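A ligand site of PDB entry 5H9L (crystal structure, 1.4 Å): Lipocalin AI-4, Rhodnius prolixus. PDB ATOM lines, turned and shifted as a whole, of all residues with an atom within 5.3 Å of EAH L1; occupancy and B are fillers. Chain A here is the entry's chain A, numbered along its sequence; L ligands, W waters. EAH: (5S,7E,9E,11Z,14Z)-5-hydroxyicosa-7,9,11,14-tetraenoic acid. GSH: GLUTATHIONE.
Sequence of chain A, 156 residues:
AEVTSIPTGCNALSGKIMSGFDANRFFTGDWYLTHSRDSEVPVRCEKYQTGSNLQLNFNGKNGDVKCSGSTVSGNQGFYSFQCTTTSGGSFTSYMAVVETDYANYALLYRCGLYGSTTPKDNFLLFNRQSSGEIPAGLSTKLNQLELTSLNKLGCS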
ATOM      1  N   PHE A  26      -2.665  10.962  -1.521  1.00  0.00           N
ATOM      2  CA  PHE A  26      -1.458  11.696  -1.885  1.00  0.00           C
ATOM      3  C   PHE A  26      -1.523  12.297  -3.305  1.00  0.00           C
ATOM      4  O   PHE A  26      -1.183  13.467  -3.515  1.00  0.00           O
ATOM      5  CB  PHE A  26      -0.209  10.811  -1.784  1.00  0.00           C
ATOM      6  CG  PHE A  26       1.023  11.503  -2.246  1.00  0.00           C
ATOM      7  CD1 PHE A  26       1.608  12.485  -1.469  1.00  0.00           C
ATOM      8  CD2 PHE A  26       1.591  11.227  -3.480  1.00  0.00           C
ATOM      9  CE1 PHE A  26       2.735  13.160  -1.908  1.00  0.00           C
ATOM     10  CE2 PHE A  26       2.716  11.880  -3.916  1.00  0.00           C
ATOM     11  CZ  PHE A  26       3.290  12.869  -3.132  1.00  0.00           C
ATOM     12  N   PHE A  27      -1.911  11.468  -4.262  1.00  0.00           N
ATOM     13  CA  PHE A  27      -1.958  11.871  -5.665  1.00  0.00           C
ATOM     14  C   PHE A  27      -3.269  12.595  -5.988  1.00  0.00           C
ATOM     15  O   PHE A  27      -4.056  12.160  -6.834  1.00  0.00           O
ATOM     16  CB  PHE A  27      -1.795  10.654  -6.571  1.00  0.00           C
ATOM     17  CG  PHE A  27      -0.428  10.013  -6.486  1.00  0.00           C
ATOM     18  CD1 PHE A  27       0.666  10.641  -7.055  1.00  0.00           C
ATOM     19  CD2 PHE A  27      -0.253   8.787  -5.855  1.00  0.00           C
ATOM     20  CE1 PHE A  27       1.928  10.062  -6.990  1.00  0.00           C
ATOM     21  CE2 PHE A  27       1.001   8.206  -5.785  1.00  0.00           C
ATOM     22  CZ  PHE A  27       2.086   8.842  -6.361  1.00  0.00           C
ATOM     23  N   TRP A  31       1.052  20.053  -5.421  1.00  0.00           N
ATOM     24  CA  TRP A  31       2.161  19.955  -4.477  1.00  0.00           C
ATOM     25  C   TRP A  31       3.290  20.889  -4.939  1.00  0.00           C
ATOM     26  O   TRP A  31       3.771  20.751  -6.068  1.00  0.00           O
ATOM     27  CB  TRP A  31       2.697  18.531  -4.407  1.00  0.00           C
ATOM     28  CG  TRP A  31       1.882  17.540  -3.606  1.00  0.00           C
ATOM     29  CD1 TRP A  31       1.128  16.517  -4.097  1.00  0.00           C
ATOM     30  CD2 TRP A  31       1.791  17.448  -2.175  1.00  0.00           C
ATOM     31  NE1 TRP A  31       0.556  15.810  -3.074  1.00  0.00           N
ATOM     32  CE2 TRP A  31       0.959  16.349  -1.884  1.00  0.00           C
ATOM     33  CE3 TRP A  31       2.346  18.183  -1.128  1.00  0.00           C
ATOM     34  CZ2 TRP A  31       0.654  15.967  -0.562  1.00  0.00           C
ATOM     35  CZ3 TRP A  31       2.048  17.816   0.176  1.00  0.00           C
ATOM     36  CH2 TRP A  31       1.214  16.719   0.444  1.00  0.00           C
ATOM     37  N   GLU A  40      19.727  22.966  -7.559  1.00  0.00           N
ATOM     38  CA  GLU A  40      20.369  23.614  -8.684  1.00  0.00           C
ATOM     39  C   GLU A  40      20.391  25.110  -8.469  1.00  0.00           C
ATOM     40  O   GLU A  40      19.755  25.626  -7.536  1.00  0.00           O
ATOM     41  CB  GLU A  40      19.608  23.311  -9.981  1.00  0.00           C
ATOM     42  CG  GLU A  40      19.205  21.865 -10.175  1.00  0.00           C
ATOM     43  CD  GLU A  40      18.116  21.718 -11.219  1.00  0.00           C
ATOM     44  OE1 GLU A  40      17.401  22.714 -11.469  1.00  0.00           O
ATOM     45  OE2 GLU A  40      17.966  20.617 -11.781  1.00  0.00           O
ATOM     46  N   TYR A  48       3.662  20.817  -8.846  1.00  0.00           N
ATOM     47  CA  TYR A  48       3.270  19.527  -9.387  1.00  0.00           C
ATOM     48  C   TYR A  48       1.756  19.387  -9.304  1.00  0.00           C
ATOM     49  O   TYR A  48       1.177  19.340  -8.226  1.00  0.00           O
ATOM     50  CB  TYR A  48       3.997  18.404  -8.627  1.00  0.00           C
ATOM     51  CG  TYR A  48       5.471  18.310  -8.963  1.00  0.00           C
ATOM     52  CD1 TYR A  48       6.374  19.271  -8.518  1.00  0.00           C
ATOM     53  CD2 TYR A  48       5.970  17.236  -9.708  1.00  0.00           C
ATOM     54  CE1 TYR A  48       7.736  19.179  -8.828  1.00  0.00           C
ATOM     55  CE2 TYR A  48       7.324  17.140 -10.013  1.00  0.00           C
ATOM     56  CZ  TYR A  48       8.198  18.103  -9.572  1.00  0.00           C
ATOM     57  OH  TYR A  48       9.538  18.015  -9.892  1.00  0.00           O
ATOM     58  N   THR A  50      -1.557  17.148  -9.969  1.00  0.00           N
ATOM     59  CA  THR A  50      -1.902  15.735 -10.095  1.00  0.00           C
ATOM     60  C   THR A  50      -3.278  15.556 -10.740  1.00  0.00           C
ATOM     61  O   THR A  50      -4.164  16.424 -10.612  1.00  0.00           O
ATOM     62  CB  THR A  50      -1.931  15.014  -8.734  1.00  0.00           C
ATOM     63  OG1 THR A  50      -3.050  15.477  -7.968  1.00  0.00           O
ATOM     64  CG2 THR A  50      -0.635  15.246  -7.968  1.00  0.00           C
ATOM     65  N   LEU A  56       0.662  13.369 -13.888  1.00  0.00           N
ATOM     66  CA  LEU A  56       1.050  14.641 -13.307  1.00  0.00           C
ATOM     67  C   LEU A  56       1.635  15.566 -14.346  1.00  0.00           C
ATOM     68  O   LEU A  56       2.049  15.167 -15.431  1.00  0.00           O
ATOM     69  CB  LEU A  56       2.007  14.430 -12.131  1.00  0.00           C
ATOM     70  CG  LEU A  56       3.373  13.762 -12.248  1.00  0.00           C
ATOM     71  CD1 LEU A  56       4.430  14.748 -12.728  1.00  0.00           C
ATOM     72  CD2 LEU A  56       3.768  13.173 -10.904  1.00  0.00           C
ATOM     73  N   PHE A  58       4.099  19.254 -14.400  1.00  0.00           N
ATOM     74  CA  PHE A  58       4.770  20.310 -13.640  1.00  0.00           C
ATOM     75  C   PHE A  58       5.541  21.226 -14.549  1.00  0.00           C
ATOM     76  O   PHE A  58       5.849  20.895 -15.689  1.00  0.00           O
ATOM     77  CB  PHE A  58       5.685  19.725 -12.547  1.00  0.00           C
ATOM     78  CG  PHE A  58       6.917  19.012 -13.065  1.00  0.00           C
ATOM     79  CD1 PHE A  58       6.860  17.668 -13.402  1.00  0.00           C
ATOM     80  CD2 PHE A  58       8.143  19.663 -13.157  1.00  0.00           C
ATOM     81  CE1 PHE A  58       7.984  16.997 -13.864  1.00  0.00           C
ATOM     82  CE2 PHE A  58       9.278  18.993 -13.602  1.00  0.00           C
ATOM     83  CZ  PHE A  58       9.188  17.653 -13.966  1.00  0.00           C
ATOM     84  N   LYS A  61      12.386  22.788 -15.820  1.00  0.00           N
ATOM     85  CA  LYS A  61      13.503  23.710 -16.069  1.00  0.00           C
ATOM     86  C   LYS A  61      13.338  24.514 -17.344  1.00  0.00           C
ATOM     87  O   LYS A  61      13.669  25.702 -17.392  1.00  0.00           O
ATOM     88  CB  LYS A  61      14.823  22.942 -16.110  1.00  0.00           C
ATOM     89  CG  LYS A  61      15.422  22.663 -14.749  1.00  0.00           C
ATOM     90  CD  LYS A  61      16.544  21.642 -14.817  1.00  0.00           C
ATOM     91  CE  LYS A  61      16.015  20.263 -15.185  1.00  0.00           C
ATOM     92  NZ  LYS A  61      17.065  19.211 -15.118  1.00  0.00           N
ATOM     93  N   CYS A  67       3.878  13.589 -16.982  1.00  0.00           N
ATOM     94  CA  CYS A  67       4.343  12.283 -16.538  1.00  0.00           C
ATOM     95  C   CYS A  67       3.204  11.311 -16.295  1.00  0.00           C
ATOM     96  O   CYS A  67       2.098  11.700 -15.904  1.00  0.00           O
ATOM     97  CB  CYS A  67       5.165  12.375 -15.262  1.00  0.00           C
ATOM     98  SG  CYS A  67       6.607  13.474 -15.310  1.00  0.00           S
ATOM     99  N   PHE A  81       7.803   6.874 -13.064  1.00  0.00           N
ATOM    100  CA  PHE A  81       7.148   7.853 -13.919  1.00  0.00           C
ATOM    101  C   PHE A  81       7.833   7.993 -15.269  1.00  0.00           C
ATOM    102  O   PHE A  81       9.049   8.152 -15.359  1.00  0.00           O
ATOM    103  CB  PHE A  81       7.074   9.222 -13.219  1.00  0.00           C
ATOM    104  CG  PHE A  81       6.000   9.293 -12.183  1.00  0.00           C
ATOM    105  CD1 PHE A  81       6.243   8.882 -10.874  1.00  0.00           C
ATOM    106  CD2 PHE A  81       4.723   9.710 -12.513  1.00  0.00           C
ATOM    107  CE1 PHE A  81       5.219   8.916  -9.917  1.00  0.00           C
ATOM    108  CE2 PHE A  81       3.708   9.748 -11.561  1.00  0.00           C
ATOM    109  CZ  PHE A  81       3.952   9.339 -10.266  1.00  0.00           C
ATOM    110  N   CYS A  83       8.097  10.416 -18.324  1.00  0.00           N
ATOM    111  CA  CYS A  83       7.873  11.851 -18.494  1.00  0.00           C
ATOM    112  C   CYS A  83       8.284  12.330 -19.883  1.00  0.00           C
ATOM    113  O   CYS A  83       9.246  11.834 -20.470  1.00  0.00           O
ATOM    114  CB  CYS A  83       8.637  12.645 -17.447  1.00  0.00           C
ATOM    115  SG  CYS A  83       8.226  12.260 -15.728  1.00  0.00           S
ATOM    116  N   PHE A  91      12.071  10.951 -20.373  1.00  0.00           N
ATOM    117  CA  PHE A  91      12.896  10.313 -19.348  1.00  0.00           C
ATOM    118  C   PHE A  91      12.056   9.524 -18.368  1.00  0.00           C
ATOM    119  O   PHE A  91      10.840   9.686 -18.306  1.00  0.00           O
ATOM    120  CB  PHE A  91      13.746  11.367 -18.610  1.00  0.00           C
ATOM    121  CG  PHE A  91      12.951  12.370 -17.830  1.00  0.00           C
ATOM    122  CD1 PHE A  91      12.483  13.528 -18.441  1.00  0.00           C
ATOM    123  CD2 PHE A  91      12.699  12.173 -16.488  1.00  0.00           C
ATOM    124  CE1 PHE A  91      11.768  14.459 -17.720  1.00  0.00           C
ATOM    125  CE2 PHE A  91      11.974  13.099 -15.748  1.00  0.00           C
ATOM    126  CZ  PHE A  91      11.511  14.249 -16.373  1.00  0.00           C
ATOM    127  N   SER A  93      11.746   8.421 -14.181  1.00  0.00           N
ATOM    128  CA  SER A  93      12.155   8.770 -12.822  1.00  0.00           C
ATOM    129  C   SER A  93      11.406   7.911 -11.812  1.00  0.00           C
ATOM    130  O   SER A  93      10.256   7.541 -12.048  1.00  0.00           O
ATOM    131  CB  SER A  93      11.907  10.243 -12.545  1.00  0.00           C
ATOM    132  OG  SER A  93      12.491  10.657 -11.320  1.00  0.00           O
ATOM    133  N   TYR A  94      12.043   7.601 -10.690  1.00  0.00           N
ATOM    134  CA  TYR A  94      11.459   6.752  -9.659  1.00  0.00           C
ATOM    135  C   TYR A  94      11.286   7.533  -8.371  1.00  0.00           C
ATOM    136  O   TYR A  94      12.137   8.363  -8.023  1.00  0.00           O
ATOM    137  CB  TYR A  94      12.346   5.536  -9.408  1.00  0.00           C
ATOM    138  CG  TYR A  94      12.509   4.670 -10.634  1.00  0.00           C
ATOM    139  CD1 TYR A  94      13.430   5.000 -11.627  1.00  0.00           C
ATOM    140  CD2 TYR A  94      11.715   3.541 -10.823  1.00  0.00           C
ATOM    141  CE1 TYR A  94      13.567   4.229 -12.760  1.00  0.00           C
ATOM    142  CE2 TYR A  94      11.850   2.767 -11.942  1.00  0.00           C
ATOM    143  CZ  TYR A  94      12.777   3.105 -12.904  1.00  0.00           C
ATOM    144  OH  TYR A  94      12.908   2.334 -14.045  1.00  0.00           O
ATOM    145  N   MET A  95      10.209   7.282  -7.642  1.00  0.00           N
ATOM    146  CA  MET A  95       9.994   7.967  -6.378  1.00  0.00           C
ATOM    147  C   MET A  95       9.275   7.114  -5.340  1.00  0.00           C
ATOM    148  O   MET A  95       8.568   6.184  -5.690  1.00  0.00           O
ATOM    149  CB  MET A  95       9.196   9.252  -6.609  1.00  0.00           C
ATOM    150  CG  MET A  95       7.846   9.012  -7.291  1.00  0.00           C
ATOM    151  SD  MET A  95       6.488   9.935  -6.586  1.00  0.00           S
ATOM    152  CE  MET A  95       6.794   9.202  -5.014  1.00  0.00           C
ATOM    153  N   LEU A 108       9.675  13.138   0.044  1.00  0.00           N
ATOM    154  CA  LEU A 108       9.850  12.101  -0.993  1.00  0.00           C
ATOM    155  C   LEU A 108      11.298  11.807  -1.246  1.00  0.00           C
ATOM    156  O   LEU A 108      12.163  12.659  -1.031  1.00  0.00           O
ATOM    157  CB  LEU A 108       9.194  12.535  -2.305  1.00  0.00           C
ATOM    158  CG  LEU A 108       7.709  12.232  -2.518  1.00  0.00           C
ATOM    159  CD1 LEU A 108       6.870  12.928  -1.452  1.00  0.00           C
ATOM    160  CD2 LEU A 108       7.253  12.637  -3.913  1.00  0.00           C
ATOM    161  N   ARG A 110      13.595  10.565  -4.575  1.00  0.00           N
ATOM    162  CA  ARG A 110      13.505  10.473  -6.026  1.00  0.00           C
ATOM    163  C   ARG A 110      14.857   9.991  -6.547  1.00  0.00           C
ATOM    164  O   ARG A 110      15.894  10.395  -6.046  1.00  0.00           O
ATOM    165  CB  ARG A 110      13.119  11.817  -6.646  1.00  0.00           C
ATOM    166  CG  ARG A 110      12.903  11.754  -8.148  1.00  0.00           C
ATOM    167  CD  ARG A 110      12.182  12.970  -8.715  1.00  0.00           C
ATOM    168  NE  ARG A 110      12.980  14.170  -8.570  1.00  0.00           N
ATOM    169  CZ  ARG A 110      12.511  15.410  -8.765  1.00  0.00           C
ATOM    170  NH1 ARG A 110      11.248  15.609  -9.096  1.00  0.00           N
ATOM    171  NH2 ARG A 110      13.315  16.450  -8.597  1.00  0.00           N
ATOM    172  N   CYS A 111      14.844   9.133  -7.560  1.00  0.00           N
ATOM    173  CA  CYS A 111      16.082   8.596  -8.110  1.00  0.00           C
ATOM    174  C   CYS A 111      15.894   8.206  -9.565  1.00  0.00           C
ATOM    175  O   CYS A 111      14.800   7.824  -9.970  1.00  0.00           O
ATOM    176  CB  CYS A 111      16.542   7.386  -7.285  1.00  0.00           C
ATOM    177  SG  CYS A 111      18.185   6.698  -7.682  1.00  0.00           S
ATOM    178  N   TYR A 114      18.776   8.572 -15.801  1.00  0.00           N
ATOM    179  CA  TYR A 114      18.747   9.656 -16.769  1.00  0.00           C
ATOM    180  C   TYR A 114      19.856   9.524 -17.811  1.00  0.00           C
ATOM    181  O   TYR A 114      20.576  10.483 -18.123  1.00  0.00           O
ATOM    182  CB  TYR A 114      18.845  11.016 -16.051  1.00  0.00           C
ATOM    183  CG  TYR A 114      17.891  11.119 -14.881  1.00  0.00           C
ATOM    184  CD1 TYR A 114      16.512  11.136 -15.083  1.00  0.00           C
ATOM    185  CD2 TYR A 114      18.363  11.157 -13.584  1.00  0.00           C
ATOM    186  CE1 TYR A 114      15.632  11.212 -14.008  1.00  0.00           C
ATOM    187  CE2 TYR A 114      17.491  11.224 -12.502  1.00  0.00           C
ATOM    188  CZ  TYR A 114      16.126  11.259 -12.727  1.00  0.00           C
ATOM    189  OH  TYR A 114      15.249  11.319 -11.676  1.00  0.00           O
ATOM    190  N   LYS A 120      21.279   9.432 -10.025  1.00  0.00           N
ATOM    191  CA  LYS A 120      21.199  10.732  -9.375  1.00  0.00           C
ATOM    192  C   LYS A 120      19.941  10.745  -8.525  1.00  0.00           C
ATOM    193  O   LYS A 120      18.845  10.492  -9.037  1.00  0.00           O
ATOM    194  CB  LYS A 120      21.176  11.877 -10.390  1.00  0.00           C
ATOM    195  CG  LYS A 120      22.404  11.965 -11.277  1.00  0.00           C
ATOM    196  CD  LYS A 120      22.532  13.303 -11.999  1.00  0.00           C
ATOM    197  CE  LYS A 120      21.231  14.095 -12.009  1.00  0.00           C
ATOM    198  NZ  LYS A 120      21.454  15.487 -12.510  1.00  0.00           N
ATOM    199  N   ASP A 121      20.089  10.984  -7.234  1.00  0.00           N
ATOM    200  CA  ASP A 121      18.919  10.917  -6.363  1.00  0.00           C
ATOM    201  C   ASP A 121      18.793  12.174  -5.510  1.00  0.00           C
ATOM    202  O   ASP A 121      19.647  13.059  -5.567  1.00  0.00           O
ATOM    203  CB  ASP A 121      18.934   9.629  -5.500  1.00  0.00           C
ATOM    204  CG  ASP A 121      20.058   9.580  -4.485  1.00  0.00           C
ATOM    205  OD1 ASP A 121      20.841  10.544  -4.358  1.00  0.00           O
ATOM    206  OD2 ASP A 121      20.161   8.545  -3.787  1.00  0.00           O
ATOM    207  N   ASN A 122      17.721  12.247  -4.728  1.00  0.00           N
ATOM    208  CA  ASN A 122      17.459  13.447  -3.937  1.00  0.00           C
ATOM    209  C   ASN A 122      16.393  13.149  -2.910  1.00  0.00           C
ATOM    210  O   ASN A 122      15.596  12.232  -3.104  1.00  0.00           O
ATOM    211  CB  ASN A 122      16.984  14.607  -4.831  1.00  0.00           C
ATOM    212  CG  ASN A 122      17.456  15.973  -4.351  1.00  0.00           C
ATOM    213  OD1 ASN A 122      17.908  16.144  -3.221  1.00  0.00           O
ATOM    214  ND2 ASN A 122      17.338  16.963  -5.228  1.00  0.00           N
ATOM    215  N   LEU A 124      13.191  15.278  -1.250  1.00  0.00           N
ATOM    216  CA  LEU A 124      12.373  16.404  -1.696  1.00  0.00           C
ATOM    217  C   LEU A 124      11.318  16.682  -0.655  1.00  0.00           C
ATOM    218  O   LEU A 124      10.646  15.762  -0.197  1.00  0.00           O
ATOM    219  CB  LEU A 124      11.684  16.087  -3.028  1.00  0.00           C
ATOM    220  CG  LEU A 124      12.578  15.589  -4.172  1.00  0.00           C
ATOM    221  CD1 LEU A 124      11.725  15.201  -5.376  1.00  0.00           C
ATOM    222  CD2 LEU A 124      13.590  16.632  -4.553  1.00  0.00           C
ATOM    223  N   PHE A 126       7.806  18.514  -0.329  1.00  0.00           N
ATOM    224  CA  PHE A 126       6.655  19.142  -0.979  1.00  0.00           C
ATOM    225  C   PHE A 126       5.709  19.711   0.061  1.00  0.00           C
ATOM    226  O   PHE A 126       5.548  19.182   1.167  1.00  0.00           O
ATOM    227  CB  PHE A 126       5.911  18.131  -1.852  1.00  0.00           C
ATOM    228  CG  PHE A 126       6.687  17.665  -3.052  1.00  0.00           C
ATOM    229  CD1 PHE A 126       7.617  16.631  -2.942  1.00  0.00           C
ATOM    230  CD2 PHE A 126       6.491  18.253  -4.299  1.00  0.00           C
ATOM    231  CE1 PHE A 126       8.323  16.217  -4.063  1.00  0.00           C
ATOM    232  CE2 PHE A 126       7.197  17.846  -5.397  1.00  0.00           C
ATOM    233  CZ  PHE A 126       8.103  16.815  -5.283  1.00  0.00           C
HETATM  234  O1  EAH L   1      16.040  16.147  -7.761  1.00  0.00           O
HETATM  235  C1  EAH L   1      16.484  15.037  -8.129  1.00  0.00           C
HETATM  236  O2  EAH L   1      15.730  14.039  -8.164  1.00  0.00           O
HETATM  237  C2  EAH L   1      17.950  14.905  -8.517  1.00  0.00           C
HETATM  238  C3  EAH L   1      18.076  14.858 -10.019  1.00  0.00           C
HETATM  239  C4  EAH L   1      17.508  16.134 -10.572  1.00  0.00           C
HETATM  240  C5  EAH L   1      17.005  15.877 -11.974  1.00  0.00           C
HETATM  241  O3  EAH L   1      16.808  17.107 -12.615  1.00  0.00           O
HETATM  242  C6  EAH L   1      15.785  15.233 -11.923  1.00  0.00           C
HETATM  243  C7  EAH L   1      14.527  15.360 -12.493  1.00  0.00           C
HETATM  244  C8  EAH L   1      13.564  14.457 -12.252  1.00  0.00           C
HETATM  245  C9  EAH L   1      12.125  14.902 -12.392  1.00  0.00           C
HETATM  246  C10 EAH L   1      11.115  14.045 -12.209  1.00  0.00           C
HETATM  247  C11 EAH L   1       9.716  14.610 -12.109  1.00  0.00           C
HETATM  248  C12 EAH L   1       8.609  13.862 -11.870  1.00  0.00           C
HETATM  249  C13 EAH L   1       8.614  12.363 -11.680  1.00  0.00           C
HETATM  250  C14 EAH L   1       9.178  11.977 -10.323  1.00  0.00           C
HETATM  251  C15 EAH L   1       8.528  12.169  -9.146  1.00  0.00           C
HETATM  252  C16 EAH L   1       7.145  12.789  -9.026  1.00  0.00           C
HETATM  253  C17 EAH L   1       6.933  13.286  -7.614  1.00  0.00           C
HETATM  254  C18 EAH L   1       5.815  14.300  -7.561  1.00  0.00           C
HETATM  255  C19 EAH L   1       4.631  13.774  -6.784  1.00  0.00           C
HETATM  256  C20 EAH L   1       3.653  14.901  -6.520  1.00  0.00           C
HETATM  257  N1  GSH L   2      21.903  14.181 -19.252  1.00  0.00           N
HETATM  258  CA1 GSH L   2      21.155  13.432 -20.194  1.00  0.00           C
HETATM  259  C1  GSH L   2      21.052  14.216 -21.484  1.00  0.00           C
HETATM  260  O11 GSH L   2      21.448  15.416 -21.542  1.00  0.00           O
HETATM  261  O12 GSH L   2      20.560  13.659 -22.517  1.00  0.00           O
HETATM  262  CB1 GSH L   2      19.737  13.159 -19.669  1.00  0.00           C
HETATM  263  CG1 GSH L   2      19.036  14.471 -19.305  1.00  0.00           C
HETATM  264  CD1 GSH L   2      17.635  14.208 -18.805  1.00  0.00           C
HETATM  265  OE1 GSH L   2      17.072  13.139 -18.961  1.00  0.00           O
HETATM  266  N2  GSH L   2      16.960  15.285 -18.124  1.00  0.00           N
HETATM  267  CA2 GSH L   2      15.617  15.042 -17.640  1.00  0.00           C
HETATM  268  C2  GSH L   2      14.813  16.291 -17.938  1.00  0.00           C
HETATM  269  O2  GSH L   2      14.831  16.793 -19.043  1.00  0.00           O
HETATM  270  CB2 GSH L   2      15.615  14.723 -16.200  1.00  0.00           C
HETATM  271  SG2 GSH L   2      16.728  15.790 -15.302  1.00  0.00           S
HETATM  272  N3  GSH L   2      14.038  16.909 -16.920  1.00  0.00           N
HETATM  273  CA3 GSH L   2      13.299  18.087 -17.243  1.00  0.00           C
HETATM  274  C3  GSH L   2      12.913  18.731 -15.933  1.00  0.00           C
HETATM  275  O31 GSH L   2      12.270  19.806 -15.960  1.00  0.00           O
HETATM  276  O32 GSH L   2      13.239  18.187 -14.861  1.00  0.00           O
HETATM  277  O   HOH W   1      16.374  11.688  -9.326  1.00  0.00           O
HETATM  278  O   HOH W   2      17.117  18.600  -8.046  1.00  0.00           O
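The guanidinium group (NE) of Arg 110 lies within salt-bridge range of an oxygen (O2) of EAH L1, at 2.8 Å.
The side-chain amide nitrogen (ND2) of Asn 122 lies within hydrogen-bond range of an oxygen (O1) of EAH L1.
An oxygen (O3) of EAH L1 is in hydrogen-bond range of the side-chain amino group (NZ) of Lys 61 (3.3 Å).
N of Lys 61 lies within hydrogen-bond range of O31 of GSH L2.
An oxygen (O32) of GSH L2 lies within salt-bridge range of the side-chain amino group (NZ) of Lys 61.
SG2 of GSH L2 lies close to O3 of EAH L1.
The backbone carbonyl oxygen of Arg 110 is in hydrogen-bond range of the backbone NH of Asn 122.
NH1 of Arg 110 is in hydrogen-bond range of OH of Tyr 48 (3.1 Å).
The side-chain hydroxyl (OH) of Tyr 114 sits at hydrogen-bond distance from the side-chain hydroxyl (OG) of Ser 93 (2.9 Å).
The backbone carbonyl oxygen of Ser 93 sits at hydrogen-bond distance from the backbone NH of Phe 81 (2.7 Å).
The backbone NH (N) of Cys 83 lies within hydrogen-bond range of the backbone carbonyl oxygen (O) of Phe 91 (2.8 Å).
The backbone carbonyl oxygen (O) of Leu 124 lies within hydrogen-bond range of the backbone NH (N) of Leu 108, at 2.8 Å.
NE1 of Trp 31 is in hydrogen-bond range of O of Phe 26 (3.0 Å).
The backbone NH of Cys 67 sits at hydrogen-bond distance from the backbone carbonyl oxygen of Leu 56 (2.9 Å).
Phe 26 touches EAH L1.
CD1 of Trp 31 touches C20 of EAH L1 (3.9 Å).
Glu 40 touches EAH L1.
Tyr 48 touches EAH L1.
Leu 56 touches EAH L1.
Phe 58 touches EAH L1.
Cys 67 touches EAH L1.
Phe 81 touches EAH L1.
Phe 91 touches EAH L1 (CE2 to C10, 3.8 Å).
Ser 93 touches EAH L1.
SD of Met 95 touches C17 of EAH L1, at 3.5 Å.
Leu 108 touches EAH L1.
Tyr 114 touches EAH L1 (OH to C8, 3.6 Å).
Lys 120 touches EAH L1.
Asp 121 touches EAH L1 (O to C2, 3.9 Å).
Hydrophobic or aromatic side chains within 4 Å of EAH L1: Phe 26, Trp 31, Tyr 48, Leu 56, Phe 58, Phe 81, Phe 91, Met 95 and Leu 108.
Within 4 Å of EAH L1: Phe 26, Trp 31, Glu 40, Tyr 48, Leu 56, Phe 58, Lys 61, Cys 67, Phe 81, Phe 91, Ser 93, Met 95, Leu 108, Arg 110, Tyr 114, Lys 120, Asp 121 and Asn 122.
Along chain A the residues within 4 Å of EAH L1 span positions 26 to 122.
Water W2 lies within hydrogen-bond range of O1 of EAH L1 and ND2 of Asn 122.
Water W1 lies within hydrogen-bond range of OH of Tyr 114 (2.6 Å), O2 of EAH L1 (2.7 Å), O of Lys 120 (2.8 Å) and N of Cys 111 (3.5 Å).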
